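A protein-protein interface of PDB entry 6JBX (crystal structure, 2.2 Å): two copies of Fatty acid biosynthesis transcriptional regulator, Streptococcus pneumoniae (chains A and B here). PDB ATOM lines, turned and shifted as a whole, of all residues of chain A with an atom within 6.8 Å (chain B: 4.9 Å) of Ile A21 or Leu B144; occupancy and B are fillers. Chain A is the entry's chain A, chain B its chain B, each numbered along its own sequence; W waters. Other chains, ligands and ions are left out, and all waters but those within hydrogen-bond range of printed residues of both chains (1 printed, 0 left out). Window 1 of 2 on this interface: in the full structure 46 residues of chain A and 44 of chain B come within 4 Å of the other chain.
No position is printed for both chains. Of the 15 pairs that touch across the chains among the printed residues, none has its exchanged pair printed and touching as well.
O of Lys A124 sits close to ND2 of Asn B143 (3.3 Å). The side-chain amide nitrogen of Asn B143 is in hydrogen-bond range of the backbone carbonyl oxygen of Ile A125.
Printed residues of chain B that touch a printed residue of chain A: Gly B140, Leu B141, Thr B142, Asn B143, Leu B144, Tyr B145, Phe B147 and Leu B148. Hydrophobic or aromatic side chains of chain B within 4 Å of the printed part of chain A: Leu B141, Leu B144, Tyr B145, Phe B147 and Leu B148. Of the 14 printed residues of chain A, 8 touch a printed residue of chain B. Printed residues of chain A that touch a printed residue of chain B: Tyr A17, Leu A18, Ser A20, Ile A21, Val A25, Met A121, Lys A124 and Ile A125. Hydrophobic or aromatic side chains of chain A within 4 Å of the printed part of chain B: Tyr A17, Leu A18, Ile A21, Val A25 and Met A121. Among the printed residues, no Asp or Glu carboxylate lies within 4 Å of a Lys or Arg side-chain nitrogen of the other chain.
OG1 of Thr B142 touches CE2 of Tyr A17 (3.7 Å). Tyr A17 touches Tyr B145 (CE1 to CE2, 3.5 Å). Leu A18 touches Leu B141. Ile A21 touches Leu B141. CD1 of Ile A21 touches CG of Leu B144, at 3.9 Å. Ile A21 touches Tyr B145. Val A25 touches Leu B148. CG of Met A121 touches CD1 of Leu B144, 3.9 Å away. Lys A124 touches Phe B147 (CG to CB, 3.6 Å). Ile A125 touches Gly B140.
Of chain B, only Leu B141 (3.6 Å), Leu B144 (3.9 Å) and Tyr B145 (3.8 Å) come within 4 Å of Ile A21. Phe A22 touches none of the printed residues of chain B. Leu A26 touches none of the printed residues of chain B. Printed residues of chain B within 4 Å of Ile A125: Gly B140 (3.9 Å) and Asn B143 (2.6 Å). Of the printed residues of chain A, Leu B141 touches Tyr A17, Leu A18 and Ile A21. Printed residues of chain A within 4 Å of Thr B142: Tyr A17. Of the printed residues of chain A, Asn B143 touches Lys A124 and Ile A125. Of chain A, only Ile A21 and Met A121 come within 4 Å of Leu B144. Printed residues of chain A within 4 Å of Phe B147: Met A121 (3.6 Å) and Lys A124 (3.6 Å). The nearest residue of chain B that does not touch Ile A21 is Leu B148 (4.1 Å). The nearest residue of chain A that does not touch Leu B144 is Ile A125 (4.02 Å). The nearest printed residue of chain B that does not touch Met A121 is Leu B148 (6.0 Å).
Water W1 bridges the side-chain hydroxyl (OG) of Ser A20 (2.8 Å) and the side-chain hydroxyl (OH) of Tyr B145 (3.2 Å).
O of Glu A16 sits at hydrogen-bond distance from OG of Ser A20, at 3.3 Å.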
ATOM      1  N   GLU A  16      -3.122   3.162 -16.831  1.00  0.00           N
ATOM      2  CA  GLU A  16      -4.097   4.094 -16.400  1.00  0.00           C
ATOM      3  C   GLU A  16      -4.690   3.697 -15.039  1.00  0.00           C
ATOM      4  O   GLU A  16      -4.800   4.544 -14.158  1.00  0.00           O
ATOM      5  CB  GLU A  16      -5.206   4.207 -17.429  1.00  0.00           C
ATOM      6  CG  GLU A  16      -6.284   5.156 -17.034  1.00  0.00           C
ATOM      7  CD  GLU A  16      -7.451   5.246 -18.004  1.00  0.00           C
ATOM      8  OE1 GLU A  16      -7.351   4.662 -19.140  1.00  0.00           O
ATOM      9  OE2 GLU A  16      -8.464   5.898 -17.610  1.00  0.00           O
ATOM     10  N   TYR A  17      -5.060   2.435 -14.849  1.00  0.00           N
ATOM     11  CA  TYR A  17      -5.678   2.052 -13.598  1.00  0.00           C
ATOM     12  C   TYR A  17      -4.640   2.110 -12.467  1.00  0.00           C
ATOM     13  O   TYR A  17      -4.925   2.657 -11.363  1.00  0.00           O
ATOM     14  CB  TYR A  17      -6.343   0.678 -13.707  1.00  0.00           C
ATOM     15  CG  TYR A  17      -7.599   0.647 -14.535  1.00  0.00           C
ATOM     16  CD1 TYR A  17      -8.199   1.806 -14.984  1.00  0.00           C
ATOM     17  CD2 TYR A  17      -8.222  -0.563 -14.851  1.00  0.00           C
ATOM     18  CE1 TYR A  17      -9.356   1.765 -15.747  1.00  0.00           C
ATOM     19  CE2 TYR A  17      -9.411  -0.618 -15.562  1.00  0.00           C
ATOM     20  CZ  TYR A  17      -9.977   0.551 -16.003  1.00  0.00           C
ATOM     21  OH  TYR A  17     -11.096   0.474 -16.759  1.00  0.00           O
ATOM     22  N   LEU A  18      -3.464   1.550 -12.702  1.00  0.00           N
ATOM     23  CA  LEU A  18      -2.464   1.555 -11.678  1.00  0.00           C
ATOM     24  C   LEU A  18      -2.112   3.009 -11.280  1.00  0.00           C
ATOM     25  O   LEU A  18      -1.935   3.277 -10.086  1.00  0.00           O
ATOM     26  CB  LEU A  18      -1.200   0.827 -12.147  1.00  0.00           C
ATOM     27  CG  LEU A  18      -1.349  -0.677 -12.307  1.00  0.00           C
ATOM     28  CD1 LEU A  18      -0.159  -1.242 -13.071  1.00  0.00           C
ATOM     29  CD2 LEU A  18      -1.494  -1.355 -10.956  1.00  0.00           C
ATOM     30  N   THR A  19      -1.976   3.907 -12.263  1.00  0.00           N
ATOM     31  CA  THR A  19      -1.572   5.299 -11.977  1.00  0.00           C
ATOM     32  C   THR A  19      -2.630   5.983 -11.101  1.00  0.00           C
ATOM     33  O   THR A  19      -2.247   6.743 -10.188  1.00  0.00           O
ATOM     34  CB  THR A  19      -1.397   6.136 -13.252  1.00  0.00           C
ATOM     35  OG1 THR A  19      -0.450   5.448 -14.076  1.00  0.00           O
ATOM     36  CG2 THR A  19      -0.936   7.553 -12.966  1.00  0.00           C
ATOM     37  N   SER A  20      -3.927   5.798 -11.414  1.00  0.00           N
ATOM     38  CA  SER A  20      -5.023   6.377 -10.600  1.00  0.00           C
ATOM     39  C   SER A  20      -4.948   5.869  -9.156  1.00  0.00           C
ATOM     40  O   SER A  20      -5.003   6.636  -8.208  1.00  0.00           O
ATOM     41  CB  SER A  20      -6.391   6.095 -11.148  1.00  0.00           C
ATOM     42  OG  SER A  20      -6.544   6.733 -12.407  1.00  0.00           O
ATOM     43  N   ILE A  21      -4.776   4.572  -9.020  1.00  0.00           N
ATOM     44  CA  ILE A  21      -4.746   3.945  -7.763  1.00  0.00           C
ATOM     45  C   ILE A  21      -3.559   4.476  -6.954  1.00  0.00           C
ATOM     46  O   ILE A  21      -3.772   4.917  -5.814  1.00  0.00           O
ATOM     47  CB  ILE A  21      -4.757   2.417  -7.892  1.00  0.00           C
ATOM     48  CG1 ILE A  21      -6.087   1.933  -8.475  1.00  0.00           C
ATOM     49  CG2 ILE A  21      -4.477   1.759  -6.568  1.00  0.00           C
ATOM     50  CD1 ILE A  21      -6.053   0.550  -9.055  1.00  0.00           C
ATOM     51  N   PHE A  22      -2.343   4.373  -7.478  1.00  0.00           N
ATOM     52  CA  PHE A  22      -1.204   4.818  -6.725  1.00  0.00           C
ATOM     53  C   PHE A  22      -1.233   6.323  -6.425  1.00  0.00           C
ATOM     54  O   PHE A  22      -0.820   6.674  -5.365  1.00  0.00           O
ATOM     55  CB  PHE A  22       0.133   4.441  -7.374  1.00  0.00           C
ATOM     56  CG  PHE A  22       0.499   3.013  -7.059  1.00  0.00           C
ATOM     57  CD1 PHE A  22       1.198   2.709  -5.908  1.00  0.00           C
ATOM     58  CD2 PHE A  22       0.111   1.970  -7.883  1.00  0.00           C
ATOM     59  CE1 PHE A  22       1.507   1.399  -5.597  1.00  0.00           C
ATOM     60  CE2 PHE A  22       0.399   0.653  -7.556  1.00  0.00           C
ATOM     61  CZ  PHE A  22       1.098   0.370  -6.416  1.00  0.00           C
ATOM     62  N   ASN A  23      -1.710   7.174  -7.298  1.00  0.00           N
ATOM     63  CA  ASN A  23      -1.708   8.607  -7.030  1.00  0.00           C
ATOM     64  C   ASN A  23      -2.799   8.989  -5.997  1.00  0.00           C
ATOM     65  O   ASN A  23      -2.669  10.041  -5.309  1.00  0.00           O
ATOM     66  CB  ASN A  23      -1.989   9.422  -8.297  1.00  0.00           C
ATOM     67  CG  ASN A  23      -0.827   9.482  -9.273  1.00  0.00           C
ATOM     68  OD1 ASN A  23       0.296   9.185  -8.913  1.00  0.00           O
ATOM     69  ND2 ASN A  23      -1.090   9.843 -10.516  1.00  0.00           N
ATOM     70  N   ASN A  24      -3.901   8.229  -5.914  1.00  0.00           N
ATOM     71  CA  ASN A  24      -5.050   8.763  -5.182  1.00  0.00           C
ATOM     72  C   ASN A  24      -5.457   7.934  -3.936  1.00  0.00           C
ATOM     73  O   ASN A  24      -6.245   8.434  -3.109  1.00  0.00           O
ATOM     74  CB  ASN A  24      -6.255   8.974  -6.084  1.00  0.00           C
ATOM     75  CG  ASN A  24      -6.054  10.016  -7.165  1.00  0.00           C
ATOM     76  OD1 ASN A  24      -6.692   9.930  -8.202  1.00  0.00           O
ATOM     77  ND2 ASN A  24      -5.166  10.975  -6.970  1.00  0.00           N
ATOM     78  N   VAL A  25      -5.001   6.713  -3.767  1.00  0.00           N
ATOM     79  CA  VAL A  25      -5.604   5.804  -2.778  1.00  0.00           C
ATOM     80  C   VAL A  25      -5.406   6.390  -1.367  1.00  0.00           C
ATOM     81  O   VAL A  25      -6.341   6.325  -0.577  1.00  0.00           O
ATOM     82  CB  VAL A  25      -5.047   4.381  -2.844  1.00  0.00           C
ATOM     83  CG1 VAL A  25      -3.549   4.329  -2.537  1.00  0.00           C
ATOM     84  CG2 VAL A  25      -5.844   3.455  -1.909  1.00  0.00           C
ATOM     85  N   LEU A  26      -4.235   6.967  -1.066  1.00  0.00           N
ATOM     86  CA  LEU A  26      -3.964   7.492   0.298  1.00  0.00           C
ATOM     87  C   LEU A  26      -4.790   8.762   0.554  1.00  0.00           C
ATOM     88  O   LEU A  26      -5.254   8.950   1.641  1.00  0.00           O
ATOM     89  CB  LEU A  26      -2.465   7.769   0.498  1.00  0.00           C
ATOM     90  CG  LEU A  26      -1.583   6.531   0.695  1.00  0.00           C
ATOM     91  CD1 LEU A  26      -0.195   6.890   1.181  1.00  0.00           C
ATOM     92  CD2 LEU A  26      -2.195   5.508   1.622  1.00  0.00           C
ATOM     93  N   MET A 121     -13.386  -2.264   0.643  1.00  0.00           N
ATOM     94  CA  MET A 121     -12.490  -2.265  -0.478  1.00  0.00           C
ATOM     95  C   MET A 121     -12.322  -3.694  -1.024  1.00  0.00           C
ATOM     96  O   MET A 121     -12.344  -3.912  -2.247  1.00  0.00           O
ATOM     97  CB  MET A 121     -11.110  -1.717  -0.089  1.00  0.00           C
ATOM     98  CG  MET A 121     -10.161  -1.593  -1.266  1.00  0.00           C
ATOM     99  SD  MET A 121      -8.456  -1.026  -0.790  1.00  0.00           S
ATOM    100  CE  MET A 121      -7.846  -2.490   0.029  1.00  0.00           C
ATOM    101  N   LYS A 124     -15.460  -4.813  -2.791  1.00  0.00           N
ATOM    102  CA  LYS A 124     -15.550  -4.319  -4.157  1.00  0.00           C
ATOM    103  C   LYS A 124     -14.537  -5.049  -5.050  1.00  0.00           C
ATOM    104  O   LYS A 124     -14.845  -5.375  -6.179  1.00  0.00           O
ATOM    105  CB  LYS A 124     -15.401  -2.803  -4.185  1.00  0.00           C
ATOM    106  CG  LYS A 124     -15.561  -2.191  -5.567  1.00  0.00           C
ATOM    107  CD  LYS A 124     -16.822  -2.601  -6.312  1.00  0.00           C
ATOM    108  CE  LYS A 124     -16.970  -1.795  -7.585  1.00  0.00           C
ATOM    109  NZ  LYS A 124     -18.062  -2.275  -8.445  1.00  0.00           N
ATOM    110  N   ILE A 125     -13.345  -5.343  -4.548  1.00  0.00           N
ATOM    111  CA  ILE A 125     -12.341  -6.010  -5.366  1.00  0.00           C
ATOM    112  C   ILE A 125     -12.904  -7.338  -5.896  1.00  0.00           C
ATOM    113  O   ILE A 125     -12.829  -7.582  -7.075  1.00  0.00           O
ATOM    114  CB  ILE A 125     -11.019  -6.200  -4.611  1.00  0.00           C
ATOM    115  CG1 ILE A 125     -10.321  -4.862  -4.435  1.00  0.00           C
ATOM    116  CG2 ILE A 125     -10.099  -7.162  -5.309  1.00  0.00           C
ATOM    117  CD1 ILE A 125      -9.015  -4.971  -3.705  1.00  0.00           C
ATOM    118  N   GLY B 140      -9.796  -7.854 -10.636  1.00  0.00           N
ATOM    119  CA  GLY B 140      -9.632  -7.162  -9.340  1.00  0.00           C
ATOM    120  C   GLY B 140      -9.082  -5.740  -9.524  1.00  0.00           C
ATOM    121  O   GLY B 140      -9.555  -4.790  -8.888  1.00  0.00           O
ATOM    122  N   LEU B 141      -8.145  -5.564 -10.450  1.00  0.00           N
ATOM    123  CA  LEU B 141      -7.544  -4.208 -10.690  1.00  0.00           C
ATOM    124  C   LEU B 141      -8.652  -3.273 -11.149  1.00  0.00           C
ATOM    125  O   LEU B 141      -8.749  -2.112 -10.699  1.00  0.00           O
ATOM    126  CB  LEU B 141      -6.431  -4.282 -11.734  1.00  0.00           C
ATOM    127  CG  LEU B 141      -5.797  -2.949 -12.159  1.00  0.00           C
ATOM    128  CD1 LEU B 141      -5.018  -2.309 -11.028  1.00  0.00           C
ATOM    129  CD2 LEU B 141      -4.853  -3.172 -13.338  1.00  0.00           C
ATOM    130  N   THR B 142      -9.488  -3.774 -12.049  1.00  0.00           N
ATOM    131  CA  THR B 142     -10.600  -2.970 -12.525  1.00  0.00           C
ATOM    132  C   THR B 142     -11.514  -2.595 -11.354  1.00  0.00           C
ATOM    133  O   THR B 142     -11.970  -1.432 -11.215  1.00  0.00           O
ATOM    134  CB  THR B 142     -11.361  -3.715 -13.623  1.00  0.00           C
ATOM    135  OG1 THR B 142     -10.447  -4.016 -14.679  1.00  0.00           O
ATOM    136  CG2 THR B 142     -12.510  -2.908 -14.162  1.00  0.00           C
ATOM    137  N   ASN B 143     -11.814  -3.573 -10.513  1.00  0.00           N
ATOM    138  CA  ASN B 143     -12.748  -3.343  -9.403  1.00  0.00           C
ATOM    139  C   ASN B 143     -12.151  -2.339  -8.403  1.00  0.00           C
ATOM    140  O   ASN B 143     -12.868  -1.477  -7.915  1.00  0.00           O
ATOM    141  CB  ASN B 143     -13.117  -4.646  -8.684  1.00  0.00           C
ATOM    142  CG  ASN B 143     -14.110  -5.503  -9.454  1.00  0.00           C
ATOM    143  OD1 ASN B 143     -14.807  -4.997 -10.311  1.00  0.00           O
ATOM    144  ND2 ASN B 143     -14.198  -6.788  -9.133  1.00  0.00           N
ATOM    145  N   LEU B 144     -10.869  -2.478  -8.104  1.00  0.00           N
ATOM    146  CA  LEU B 144     -10.183  -1.592  -7.189  1.00  0.00           C
ATOM    147  C   LEU B 144     -10.181  -0.193  -7.794  1.00  0.00           C
ATOM    148  O   LEU B 144     -10.542   0.792  -7.101  1.00  0.00           O
ATOM    149  CB  LEU B 144      -8.760  -2.086  -6.895  1.00  0.00           C
ATOM    150  CG  LEU B 144      -7.902  -1.138  -6.038  1.00  0.00           C
ATOM    151  CD1 LEU B 144      -8.599  -0.774  -4.738  1.00  0.00           C
ATOM    152  CD2 LEU B 144      -6.553  -1.713  -5.707  1.00  0.00           C
ATOM    153  N   TYR B 145      -9.846  -0.088  -9.081  1.00  0.00           N
ATOM    154  CA  TYR B 145      -9.905   1.208  -9.700  1.00  0.00           C
ATOM    155  C   TYR B 145     -11.296   1.825  -9.501  1.00  0.00           C
ATOM    156  O   TYR B 145     -11.428   3.008  -9.193  1.00  0.00           O
ATOM    157  CB  TYR B 145      -9.572   1.133 -11.191  1.00  0.00           C
ATOM    158  CG  TYR B 145      -9.911   2.370 -11.975  1.00  0.00           C
ATOM    159  CD1 TYR B 145      -9.054   3.464 -11.997  1.00  0.00           C
ATOM    160  CD2 TYR B 145     -11.071   2.431 -12.728  1.00  0.00           C
ATOM    161  CE1 TYR B 145      -9.366   4.609 -12.715  1.00  0.00           C
ATOM    162  CE2 TYR B 145     -11.364   3.534 -13.512  1.00  0.00           C
ATOM    163  CZ  TYR B 145     -10.504   4.621 -13.497  1.00  0.00           C
ATOM    164  OH  TYR B 145     -10.797   5.719 -14.232  1.00  0.00           O
ATOM    165  N   GLN B 146     -12.337   1.018  -9.724  1.00  0.00           N
ATOM    166  CA  GLN B 146     -13.692   1.544  -9.669  1.00  0.00           C
ATOM    167  C   GLN B 146     -14.083   1.866  -8.219  1.00  0.00           C
ATOM    168  O   GLN B 146     -14.797   2.833  -7.993  1.00  0.00           O
ATOM    169  CB  GLN B 146     -14.679   0.559 -10.283  1.00  0.00           C
ATOM    170  CG  GLN B 146     -16.064   1.135 -10.443  1.00  0.00           C
ATOM    171  CD  GLN B 146     -16.180   2.116 -11.584  1.00  0.00           C
ATOM    172  OE1 GLN B 146     -15.600   1.908 -12.646  1.00  0.00           O
ATOM    173  NE2 GLN B 146     -16.916   3.201 -11.358  1.00  0.00           N
ATOM    174  N   PHE B 147     -13.647   1.076  -7.266  1.00  0.00           N
ATOM    175  CA  PHE B 147     -13.952   1.399  -5.841  1.00  0.00           C
ATOM    176  C   PHE B 147     -13.544   2.852  -5.534  1.00  0.00           C
ATOM    177  O   PHE B 147     -14.322   3.661  -5.015  1.00  0.00           O
ATOM    178  CB  PHE B 147     -13.191   0.435  -4.934  1.00  0.00           C
ATOM    179  CG  PHE B 147     -13.287   0.724  -3.457  1.00  0.00           C
ATOM    180  CD1 PHE B 147     -14.486   0.566  -2.767  1.00  0.00           C
ATOM    181  CD2 PHE B 147     -12.177   1.160  -2.752  1.00  0.00           C
ATOM    182  CE1 PHE B 147     -14.579   0.867  -1.416  1.00  0.00           C
ATOM    183  CE2 PHE B 147     -12.263   1.440  -1.392  1.00  0.00           C
ATOM    184  CZ  PHE B 147     -13.467   1.278  -0.726  1.00  0.00           C
ATOM    185  N   LEU B 148     -12.305   3.170  -5.888  1.00  0.00           N
ATOM    186  CA  LEU B 148     -11.759   4.500  -5.635  1.00  0.00           C
ATOM    187  C   LEU B 148     -12.466   5.543  -6.475  1.00  0.00           C
ATOM    188  O   LEU B 148     -12.770   6.636  -5.931  1.00  0.00           O
ATOM    189  CB  LEU B 148     -10.252   4.501  -5.910  1.00  0.00           C
ATOM    190  CG  LEU B 148      -9.498   3.622  -4.934  1.00  0.00           C
ATOM    191  CD1 LEU B 148      -8.037   3.549  -5.289  1.00  0.00           C
ATOM    192  CD2 LEU B 148      -9.729   4.122  -3.508  1.00  0.00           C
HETATM  193  O   HOH W   1      -8.193   7.517 -14.466  1.00  0.00           O
